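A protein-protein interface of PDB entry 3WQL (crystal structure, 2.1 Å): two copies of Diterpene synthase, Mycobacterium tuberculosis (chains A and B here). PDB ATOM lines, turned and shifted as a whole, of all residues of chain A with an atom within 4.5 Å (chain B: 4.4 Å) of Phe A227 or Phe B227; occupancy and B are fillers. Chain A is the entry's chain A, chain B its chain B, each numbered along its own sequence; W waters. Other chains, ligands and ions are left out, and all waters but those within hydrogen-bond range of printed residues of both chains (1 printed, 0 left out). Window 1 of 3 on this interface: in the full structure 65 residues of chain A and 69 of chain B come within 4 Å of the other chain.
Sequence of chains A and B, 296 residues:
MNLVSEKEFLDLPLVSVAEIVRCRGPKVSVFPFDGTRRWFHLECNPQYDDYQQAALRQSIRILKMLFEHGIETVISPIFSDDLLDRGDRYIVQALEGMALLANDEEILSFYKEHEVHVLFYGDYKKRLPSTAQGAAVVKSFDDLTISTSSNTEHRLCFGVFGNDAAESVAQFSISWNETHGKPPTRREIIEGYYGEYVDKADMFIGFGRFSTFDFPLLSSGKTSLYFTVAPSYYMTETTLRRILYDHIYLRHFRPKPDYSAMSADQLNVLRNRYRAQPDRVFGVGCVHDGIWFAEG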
ATOM      1  N   GLY A 206     -12.056 -25.470 -20.038  1.00  0.00           N
ATOM      2  CA  GLY A 206     -12.695 -24.160 -20.034  1.00  0.00           C
ATOM      3  C   GLY A 206     -13.897 -24.007 -19.113  1.00  0.00           C
ATOM      4  O   GLY A 206     -14.163 -24.866 -18.266  1.00  0.00           O
ATOM      5  N   PHE A 207     -14.635 -22.913 -19.302  1.00  0.00           N
ATOM      6  CA  PHE A 207     -15.802 -22.595 -18.485  1.00  0.00           C
ATOM      7  C   PHE A 207     -16.864 -21.815 -19.262  1.00  0.00           C
ATOM      8  O   PHE A 207     -16.534 -20.913 -20.023  1.00  0.00           O
ATOM      9  CB  PHE A 207     -15.364 -21.754 -17.283  1.00  0.00           C
ATOM     10  CG  PHE A 207     -16.464 -20.892 -16.703  1.00  0.00           C
ATOM     11  CD1 PHE A 207     -17.500 -21.460 -15.963  1.00  0.00           C
ATOM     12  CD2 PHE A 207     -16.453 -19.506 -16.889  1.00  0.00           C
ATOM     13  CE1 PHE A 207     -18.518 -20.657 -15.404  1.00  0.00           C
ATOM     14  CE2 PHE A 207     -17.458 -18.696 -16.342  1.00  0.00           C
ATOM     15  CZ  PHE A 207     -18.495 -19.277 -15.594  1.00  0.00           C
ATOM     16  N   GLY A 208     -18.133 -22.159 -19.048  1.00  0.00           N
ATOM     17  CA  GLY A 208     -19.229 -21.468 -19.712  1.00  0.00           C
ATOM     18  C   GLY A 208     -19.163 -21.405 -21.228  1.00  0.00           C
ATOM     19  O   GLY A 208     -19.011 -22.429 -21.898  1.00  0.00           O
ATOM     20  N   PHE A 210     -18.171 -21.534 -24.744  1.00  0.00           N
ATOM     21  CA  PHE A 210     -17.034 -22.240 -25.321  1.00  0.00           C
ATOM     22  C   PHE A 210     -16.010 -21.305 -25.950  1.00  0.00           C
ATOM     23  O   PHE A 210     -16.276 -20.670 -26.960  1.00  0.00           O
ATOM     24  CB  PHE A 210     -17.512 -23.251 -26.369  1.00  0.00           C
ATOM     25  CG  PHE A 210     -18.454 -24.302 -25.831  1.00  0.00           C
ATOM     26  CD1 PHE A 210     -18.855 -24.299 -24.495  1.00  0.00           C
ATOM     27  CD2 PHE A 210     -18.950 -25.293 -26.672  1.00  0.00           C
ATOM     28  CE1 PHE A 210     -19.735 -25.262 -24.008  1.00  0.00           C
ATOM     29  CE2 PHE A 210     -19.839 -26.269 -26.192  1.00  0.00           C
ATOM     30  CZ  PHE A 210     -20.228 -26.245 -24.859  1.00  0.00           C
ATOM     31  N   SER A 211     -14.835 -21.228 -25.335  1.00  0.00           N
ATOM     32  CA  SER A 211     -13.756 -20.396 -25.844  1.00  0.00           C
ATOM     33  C   SER A 211     -12.470 -20.859 -25.187  1.00  0.00           C
ATOM     34  O   SER A 211     -12.489 -21.509 -24.137  1.00  0.00           O
ATOM     35  CB  SER A 211     -13.988 -18.924 -25.508  1.00  0.00           C
ATOM     36  OG  SER A 211     -13.773 -18.691 -24.128  1.00  0.00           O
ATOM     37  N   THR A 212     -11.349 -20.525 -25.807  1.00  0.00           N
ATOM     38  CA  THR A 212     -10.060 -20.915 -25.278  1.00  0.00           C
ATOM     39  C   THR A 212      -9.131 -19.734 -25.446  1.00  0.00           C
ATOM     40  O   THR A 212      -9.399 -18.824 -26.252  1.00  0.00           O
ATOM     41  CB  THR A 212      -9.497 -22.141 -26.015  1.00  0.00           C
ATOM     42  OG1 THR A 212      -9.163 -21.782 -27.357  1.00  0.00           O
ATOM     43  CG2 THR A 212     -10.531 -23.264 -26.032  1.00  0.00           C
ATOM     44  N   LEU A 225     -10.602 -30.453 -25.733  1.00  0.00           N
ATOM     45  CA  LEU A 225     -11.253 -29.285 -25.160  1.00  0.00           C
ATOM     46  C   LEU A 225     -12.453 -29.663 -24.294  1.00  0.00           C
ATOM     47  O   LEU A 225     -13.264 -30.516 -24.672  1.00  0.00           O
ATOM     48  CB  LEU A 225     -11.707 -28.336 -26.272  1.00  0.00           C
ATOM     49  CG  LEU A 225     -10.656 -27.942 -27.320  1.00  0.00           C
ATOM     50  CD1 LEU A 225     -11.279 -26.990 -28.345  1.00  0.00           C
ATOM     51  CD2 LEU A 225      -9.463 -27.301 -26.638  1.00  0.00           C
ATOM     52  N   TYR A 226     -12.556 -29.023 -23.132  1.00  0.00           N
ATOM     53  CA  TYR A 226     -13.659 -29.253 -22.191  1.00  0.00           C
ATOM     54  C   TYR A 226     -14.161 -27.897 -21.693  1.00  0.00           C
ATOM     55  O   TYR A 226     -13.403 -26.917 -21.643  1.00  0.00           O
ATOM     56  CB  TYR A 226     -13.179 -30.084 -20.992  1.00  0.00           C
ATOM     57  CG  TYR A 226     -12.628 -31.436 -21.390  1.00  0.00           C
ATOM     58  CD1 TYR A 226     -13.473 -32.529 -21.571  1.00  0.00           C
ATOM     59  CD2 TYR A 226     -11.268 -31.600 -21.663  1.00  0.00           C
ATOM     60  CE1 TYR A 226     -12.981 -33.749 -22.025  1.00  0.00           C
ATOM     61  CE2 TYR A 226     -10.765 -32.817 -22.114  1.00  0.00           C
ATOM     62  CZ  TYR A 226     -11.622 -33.885 -22.300  1.00  0.00           C
ATOM     63  OH  TYR A 226     -11.132 -35.062 -22.819  1.00  0.00           O
ATOM     64  N   PHE A 227     -15.428 -27.845 -21.303  1.00  0.00           N
ATOM     65  CA  PHE A 227     -16.017 -26.602 -20.816  1.00  0.00           C
ATOM     66  C   PHE A 227     -16.989 -26.900 -19.675  1.00  0.00           C
ATOM     67  O   PHE A 227     -18.073 -27.424 -19.907  1.00  0.00           O
ATOM     68  CB  PHE A 227     -16.749 -25.902 -21.968  1.00  0.00           C
ATOM     69  CG  PHE A 227     -15.875 -25.627 -23.155  1.00  0.00           C
ATOM     70  CD1 PHE A 227     -14.915 -24.624 -23.110  1.00  0.00           C
ATOM     71  CD2 PHE A 227     -15.985 -26.393 -24.311  1.00  0.00           C
ATOM     72  CE1 PHE A 227     -14.078 -24.387 -24.193  1.00  0.00           C
ATOM     73  CE2 PHE A 227     -15.144 -26.161 -25.406  1.00  0.00           C
ATOM     74  CZ  PHE A 227     -14.194 -25.156 -25.342  1.00  0.00           C
ATOM     75  N   THR A 228     -16.599 -26.573 -18.449  1.00  0.00           N
ATOM     76  CA  THR A 228     -17.470 -26.834 -17.311  1.00  0.00           C
ATOM     77  C   THR A 228     -18.599 -25.818 -17.279  1.00  0.00           C
ATOM     78  O   THR A 228     -18.455 -24.696 -17.778  1.00  0.00           O
ATOM     79  CB  THR A 228     -16.721 -26.743 -15.978  1.00  0.00           C
ATOM     80  OG1 THR A 228     -16.246 -25.405 -15.788  1.00  0.00           O
ATOM     81  CG2 THR A 228     -15.559 -27.711 -15.956  1.00  0.00           C
ATOM     82  N   VAL A 229     -19.720 -26.222 -16.692  1.00  0.00           N
ATOM     83  CA  VAL A 229     -20.881 -25.351 -16.574  1.00  0.00           C
ATOM     84  C   VAL A 229     -20.658 -24.372 -15.430  1.00  0.00           C
ATOM     85  O   VAL A 229     -20.836 -23.166 -15.573  1.00  0.00           O
ATOM     86  CB  VAL A 229     -22.160 -26.174 -16.288  1.00  0.00           C
ATOM     87  CG1 VAL A 229     -23.355 -25.249 -16.087  1.00  0.00           C
ATOM     88  CG2 VAL A 229     -22.424 -27.131 -17.444  1.00  0.00           C
ATOM     89  N   VAL A 281     -26.094 -28.378 -32.027  1.00  0.00           N
ATOM     90  CA  VAL A 281     -24.756 -27.806 -32.003  1.00  0.00           C
ATOM     91  C   VAL A 281     -24.325 -27.433 -30.593  1.00  0.00           C
ATOM     92  O   VAL A 281     -24.868 -26.500 -29.999  1.00  0.00           O
ATOM     93  CB  VAL A 281     -24.675 -26.513 -32.872  1.00  0.00           C
ATOM     94  CG1 VAL A 281     -23.231 -26.001 -32.924  1.00  0.00           C
ATOM     95  CG2 VAL A 281     -25.195 -26.776 -34.267  1.00  0.00           C
ATOM     96  N   PHE A 282     -23.353 -28.158 -30.052  1.00  0.00           N
ATOM     97  CA  PHE A 282     -22.862 -27.844 -28.718  1.00  0.00           C
ATOM     98  C   PHE A 282     -22.097 -26.538 -28.869  1.00  0.00           C
ATOM     99  O   PHE A 282     -21.190 -26.439 -29.706  1.00  0.00           O
ATOM    100  CB  PHE A 282     -21.945 -28.954 -28.215  1.00  0.00           C
ATOM    101  CG  PHE A 282     -22.682 -30.179 -27.775  1.00  0.00           C
ATOM    102  CD1 PHE A 282     -23.239 -30.249 -26.501  1.00  0.00           C
ATOM    103  CD2 PHE A 282     -22.850 -31.251 -28.642  1.00  0.00           C
ATOM    104  CE1 PHE A 282     -23.957 -31.375 -26.100  1.00  0.00           C
ATOM    105  CE2 PHE A 282     -23.564 -32.378 -28.252  1.00  0.00           C
ATOM    106  CZ  PHE A 282     -24.119 -32.443 -26.980  1.00  0.00           C
ATOM    107  N   GLY B 206     -16.651 -26.407 -35.285  1.00  0.00           N
ATOM    108  CA  GLY B 206     -16.049 -27.731 -35.320  1.00  0.00           C
ATOM    109  C   GLY B 206     -17.043 -28.871 -35.477  1.00  0.00           C
ATOM    110  O   GLY B 206     -18.209 -28.659 -35.792  1.00  0.00           O
ATOM    111  N   PHE B 207     -16.572 -30.089 -35.230  1.00  0.00           N
ATOM    112  CA  PHE B 207     -17.386 -31.291 -35.367  1.00  0.00           C
ATOM    113  C   PHE B 207     -16.988 -32.359 -34.353  1.00  0.00           C
ATOM    114  O   PHE B 207     -15.828 -32.474 -34.016  1.00  0.00           O
ATOM    115  CB  PHE B 207     -17.213 -31.864 -36.773  1.00  0.00           C
ATOM    116  CG  PHE B 207     -17.621 -33.301 -36.893  1.00  0.00           C
ATOM    117  CD1 PHE B 207     -18.952 -33.678 -36.740  1.00  0.00           C
ATOM    118  CD2 PHE B 207     -16.665 -34.290 -37.139  1.00  0.00           C
ATOM    119  CE1 PHE B 207     -19.330 -35.027 -36.829  1.00  0.00           C
ATOM    120  CE2 PHE B 207     -17.032 -35.640 -37.231  1.00  0.00           C
ATOM    121  CZ  PHE B 207     -18.364 -36.007 -37.075  1.00  0.00           C
ATOM    122  N   GLY B 208     -17.957 -33.142 -33.884  1.00  0.00           N
ATOM    123  CA  GLY B 208     -17.675 -34.202 -32.929  1.00  0.00           C
ATOM    124  C   GLY B 208     -16.849 -33.831 -31.706  1.00  0.00           C
ATOM    125  O   GLY B 208     -17.197 -32.913 -30.945  1.00  0.00           O
ATOM    126  N   PHE B 210     -14.622 -32.264 -29.154  1.00  0.00           N
ATOM    127  CA  PHE B 210     -14.283 -30.854 -29.032  1.00  0.00           C
ATOM    128  C   PHE B 210     -12.790 -30.585 -29.220  1.00  0.00           C
ATOM    129  O   PHE B 210     -11.976 -30.949 -28.371  1.00  0.00           O
ATOM    130  CB  PHE B 210     -14.714 -30.294 -27.661  1.00  0.00           C
ATOM    131  CG  PHE B 210     -16.212 -30.263 -27.438  1.00  0.00           C
ATOM    132  CD1 PHE B 210     -17.091 -30.893 -28.314  1.00  0.00           C
ATOM    133  CD2 PHE B 210     -16.734 -29.620 -26.321  1.00  0.00           C
ATOM    134  CE1 PHE B 210     -18.466 -30.884 -28.074  1.00  0.00           C
ATOM    135  CE2 PHE B 210     -18.108 -29.607 -26.075  1.00  0.00           C
ATOM    136  CZ  PHE B 210     -18.970 -30.238 -26.948  1.00  0.00           C
ATOM    137  N   SER B 211     -12.446 -29.935 -30.330  1.00  0.00           N
ATOM    138  CA  SER B 211     -11.057 -29.570 -30.630  1.00  0.00           C
ATOM    139  C   SER B 211     -11.062 -28.607 -31.810  1.00  0.00           C
ATOM    140  O   SER B 211     -11.969 -28.640 -32.627  1.00  0.00           O
ATOM    141  CB  SER B 211     -10.229 -30.803 -30.994  1.00  0.00           C
ATOM    142  OG  SER B 211     -10.499 -31.198 -32.326  1.00  0.00           O
ATOM    143  N   THR B 212     -10.055 -27.744 -31.884  1.00  0.00           N
ATOM    144  CA  THR B 212      -9.944 -26.776 -32.974  1.00  0.00           C
ATOM    145  C   THR B 212      -8.540 -26.876 -33.544  1.00  0.00           C
ATOM    146  O   THR B 212      -7.620 -27.343 -32.871  1.00  0.00           O
ATOM    147  CB  THR B 212     -10.151 -25.324 -32.493  1.00  0.00           C
ATOM    148  OG1 THR B 212      -9.062 -24.956 -31.647  1.00  0.00           O
ATOM    149  CG2 THR B 212     -11.449 -25.192 -31.720  1.00  0.00           C
ATOM    150  N   LEU B 225     -16.664 -20.686 -30.002  1.00  0.00           N
ATOM    151  CA  LEU B 225     -16.465 -22.070 -30.425  1.00  0.00           C
ATOM    152  C   LEU B 225     -17.748 -22.893 -30.426  1.00  0.00           C
ATOM    153  O   LEU B 225     -18.490 -22.895 -29.439  1.00  0.00           O
ATOM    154  CB  LEU B 225     -15.427 -22.745 -29.513  1.00  0.00           C
ATOM    155  CG  LEU B 225     -14.083 -22.032 -29.320  1.00  0.00           C
ATOM    156  CD1 LEU B 225     -13.153 -22.928 -28.507  1.00  0.00           C
ATOM    157  CD2 LEU B 225     -13.461 -21.719 -30.662  1.00  0.00           C
ATOM    158  N   TYR B 226     -17.979 -23.609 -31.527  1.00  0.00           N
ATOM    159  CA  TYR B 226     -19.157 -24.452 -31.706  1.00  0.00           C
ATOM    160  C   TYR B 226     -18.738 -25.832 -32.207  1.00  0.00           C
ATOM    161  O   TYR B 226     -17.768 -25.969 -32.953  1.00  0.00           O
ATOM    162  CB  TYR B 226     -20.102 -23.823 -32.726  1.00  0.00           C
ATOM    163  CG  TYR B 226     -20.530 -22.425 -32.352  1.00  0.00           C
ATOM    164  CD1 TYR B 226     -21.675 -22.206 -31.580  1.00  0.00           C
ATOM    165  CD2 TYR B 226     -19.762 -21.320 -32.725  1.00  0.00           C
ATOM    166  CE1 TYR B 226     -22.042 -20.920 -31.190  1.00  0.00           C
ATOM    167  CE2 TYR B 226     -20.120 -20.036 -32.341  1.00  0.00           C
ATOM    168  CZ  TYR B 226     -21.264 -19.845 -31.572  1.00  0.00           C
ATOM    169  OH  TYR B 226     -21.623 -18.577 -31.190  1.00  0.00           O
ATOM    170  N   PHE B 227     -19.468 -26.859 -31.799  1.00  0.00           N
ATOM    171  CA  PHE B 227     -19.150 -28.207 -32.237  1.00  0.00           C
ATOM    172  C   PHE B 227     -20.427 -28.933 -32.644  1.00  0.00           C
ATOM    173  O   PHE B 227     -21.252 -29.286 -31.802  1.00  0.00           O
ATOM    174  CB  PHE B 227     -18.423 -28.948 -31.113  1.00  0.00           C
ATOM    175  CG  PHE B 227     -17.148 -28.267 -30.675  1.00  0.00           C
ATOM    176  CD1 PHE B 227     -16.004 -28.319 -31.475  1.00  0.00           C
ATOM    177  CD2 PHE B 227     -17.117 -27.506 -29.510  1.00  0.00           C
ATOM    178  CE1 PHE B 227     -14.850 -27.613 -31.127  1.00  0.00           C
ATOM    179  CE2 PHE B 227     -15.974 -26.800 -29.154  1.00  0.00           C
ATOM    180  CZ  PHE B 227     -14.837 -26.853 -29.968  1.00  0.00           C
ATOM    181  N   THR B 228     -20.594 -29.136 -33.942  1.00  0.00           N
ATOM    182  CA  THR B 228     -21.775 -29.819 -34.444  1.00  0.00           C
ATOM    183  C   THR B 228     -21.678 -31.289 -34.103  1.00  0.00           C
ATOM    184  O   THR B 228     -20.585 -31.824 -33.966  1.00  0.00           O
ATOM    185  CB  THR B 228     -21.913 -29.699 -35.976  1.00  0.00           C
ATOM    186  OG1 THR B 228     -20.811 -30.359 -36.613  1.00  0.00           O
ATOM    187  CG2 THR B 228     -21.940 -28.239 -36.392  1.00  0.00           C
ATOM    188  N   VAL B 229     -22.832 -31.934 -33.962  1.00  0.00           N
ATOM    189  CA  VAL B 229     -22.883 -33.357 -33.667  1.00  0.00           C
ATOM    190  C   VAL B 229     -22.723 -34.115 -34.977  1.00  0.00           C
ATOM    191  O   VAL B 229     -21.944 -35.059 -35.069  1.00  0.00           O
ATOM    192  CB  VAL B 229     -24.232 -33.743 -33.029  1.00  0.00           C
ATOM    193  CG1 VAL B 229     -24.380 -35.259 -32.997  1.00  0.00           C
ATOM    194  CG2 VAL B 229     -24.322 -33.153 -31.619  1.00  0.00           C
ATOM    195  N   VAL B 281     -19.674 -31.504 -17.458  1.00  0.00           N
ATOM    196  CA  VAL B 281     -18.705 -30.878 -18.349  1.00  0.00           C
ATOM    197  C   VAL B 281     -18.931 -31.193 -19.824  1.00  0.00           C
ATOM    198  O   VAL B 281     -18.869 -32.356 -20.244  1.00  0.00           O
ATOM    199  CB  VAL B 281     -17.265 -31.318 -17.982  1.00  0.00           C
ATOM    200  CG1 VAL B 281     -16.253 -30.536 -18.806  1.00  0.00           C
ATOM    201  CG2 VAL B 281     -17.021 -31.125 -16.488  1.00  0.00           C
ATOM    202  N   PHE B 282     -19.191 -30.153 -20.609  1.00  0.00           N
ATOM    203  CA  PHE B 282     -19.378 -30.311 -22.043  1.00  0.00           C
ATOM    204  C   PHE B 282     -18.001 -30.630 -22.612  1.00  0.00           C
ATOM    205  O   PHE B 282     -17.034 -29.922 -22.350  1.00  0.00           O
ATOM    206  CB  PHE B 282     -19.955 -29.022 -22.634  1.00  0.00           C
ATOM    207  CG  PHE B 282     -21.403 -28.826 -22.307  1.00  0.00           C
ATOM    208  CD1 PHE B 282     -22.381 -29.553 -22.983  1.00  0.00           C
ATOM    209  CD2 PHE B 282     -21.791 -27.981 -21.271  1.00  0.00           C
ATOM    210  CE1 PHE B 282     -23.729 -29.448 -22.627  1.00  0.00           C
ATOM    211  CE2 PHE B 282     -23.140 -27.866 -20.900  1.00  0.00           C
ATOM    212  CZ  PHE B 282     -24.110 -28.600 -21.575  1.00  0.00           C
HETATM  213  O   HOH W   1      -7.851 -23.732 -28.628  1.00  0.00           O
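Water W1 lies within hydrogen-bond range of the side-chain hydroxyl (OG1) of Thr A212 (2.7 Å) and the side-chain hydroxyl (OG1) of Thr B212 (3.5 Å).
Thr A212 touches Leu B225, and with the chains exchanged Leu A225 touches Thr B212.
Tyr A226 touches Val B281, and with the chains exchanged Val A281 touches Tyr B226.
Phe A227 touches Phe B210, but with the chains exchanged Phe A210 does not touch Phe B227 (4.04 Å).
Phe A227 touches Val B281, and with the chains exchanged Val A281 touches Phe B227.
Positions printed for both chains: 206, 207, 208, 210, 211, 212, 225, 226, 227, 228, 229, 281 and 282.
Of the 24 pairs that touch across the chains among the printed residues, 21 have their exchanged pair printed and touching as well.
The backbone NH (N) of Gly A208 lies within hydrogen-bond range of the backbone carbonyl oxygen (O) of Thr A228 (2.9 Å).
The backbone carbonyl oxygen of Tyr A226 lies within hydrogen-bond range of the backbone NH of Gly A206.
The backbone carbonyl oxygen (O) of Gly A206 lies within hydrogen-bond range of the backbone NH (N) of Thr A228 (3.0 Å).
The backbone NH (N) of Gly B206 is in hydrogen-bond range of the backbone carbonyl oxygen (O) of Tyr B226.
Of the printed residues of chain B, Phe A227 touches Phe B210 (3.9 Å), Phe B227 (3.9 Å), Val B281 (3.8 Å) and Phe B282 (2.8 Å).
Of the printed residues of chain A, Thr B212 touches Leu A225 (3.8 Å).
Of chain A, only Leu A225 (3.9 Å), Phe A227 (3.9 Å), Val A281 (3.8 Å) and Phe A282 (2.7 Å) come within 4 Å of Phe B227.
Printed residues of chain A within 4 Å of Phe B282: Phe A210, Tyr A226, Phe A227, Val A229 and Phe A282.
Among the printed residues, merely in contact across the chains: Phe A210 with Phe B210, Phe A210 with Phe B282, Ser A211 with Leu B225, Thr A212 with Leu B225, Leu A225 with Ser B211, Leu A225 with Thr B212, Leu A225 with Phe B227, Tyr A226 with Val B281, Tyr A226 with Phe B282, Phe A227 with Phe B210, Phe A227 with Phe B227, Phe A227 with Val B281, Thr A228 with Val B281, Val A229 with Phe B282, Val A281 with Tyr B226, Val A281 with Phe B227, Phe A282 with Phe B210, Phe A282 with Tyr B226, Phe A282 with Val B229 and Phe A282 with Phe B282.
Of the 13 printed residues of chain A, 10 touch a printed residue of chain B.
Printed residues of chain A that touch a printed residue of chain B: Phe A210, Ser A211, Thr A212, Leu A225, Tyr A226, Phe A227, Thr A228, Val A229, Val A281 and Phe A282.
Hydrophobic or aromatic side chains of chain A within 4 Å of the printed part of chain B: Phe A210, Leu A225, Tyr A226, Phe A227, Val A229, Val A281 and Phe A282.
Among the printed residues, 24 pairs touch across the chains.
N of Phe B227 lies within hydrogen-bond range of O of Phe A282, 2.7 Å away.
The backbone carbonyl oxygen (O) of Phe A210 lies within hydrogen-bond range of the backbone NH (N) of Leu B225 (3.1 Å).
The backbone carbonyl oxygen (O) of Phe B282 is in hydrogen-bond range of the backbone NH (N) of Phe A227 (2.8 Å).
The backbone NH (N) of Leu A225 is in hydrogen-bond range of the backbone carbonyl oxygen (O) of Phe B210.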
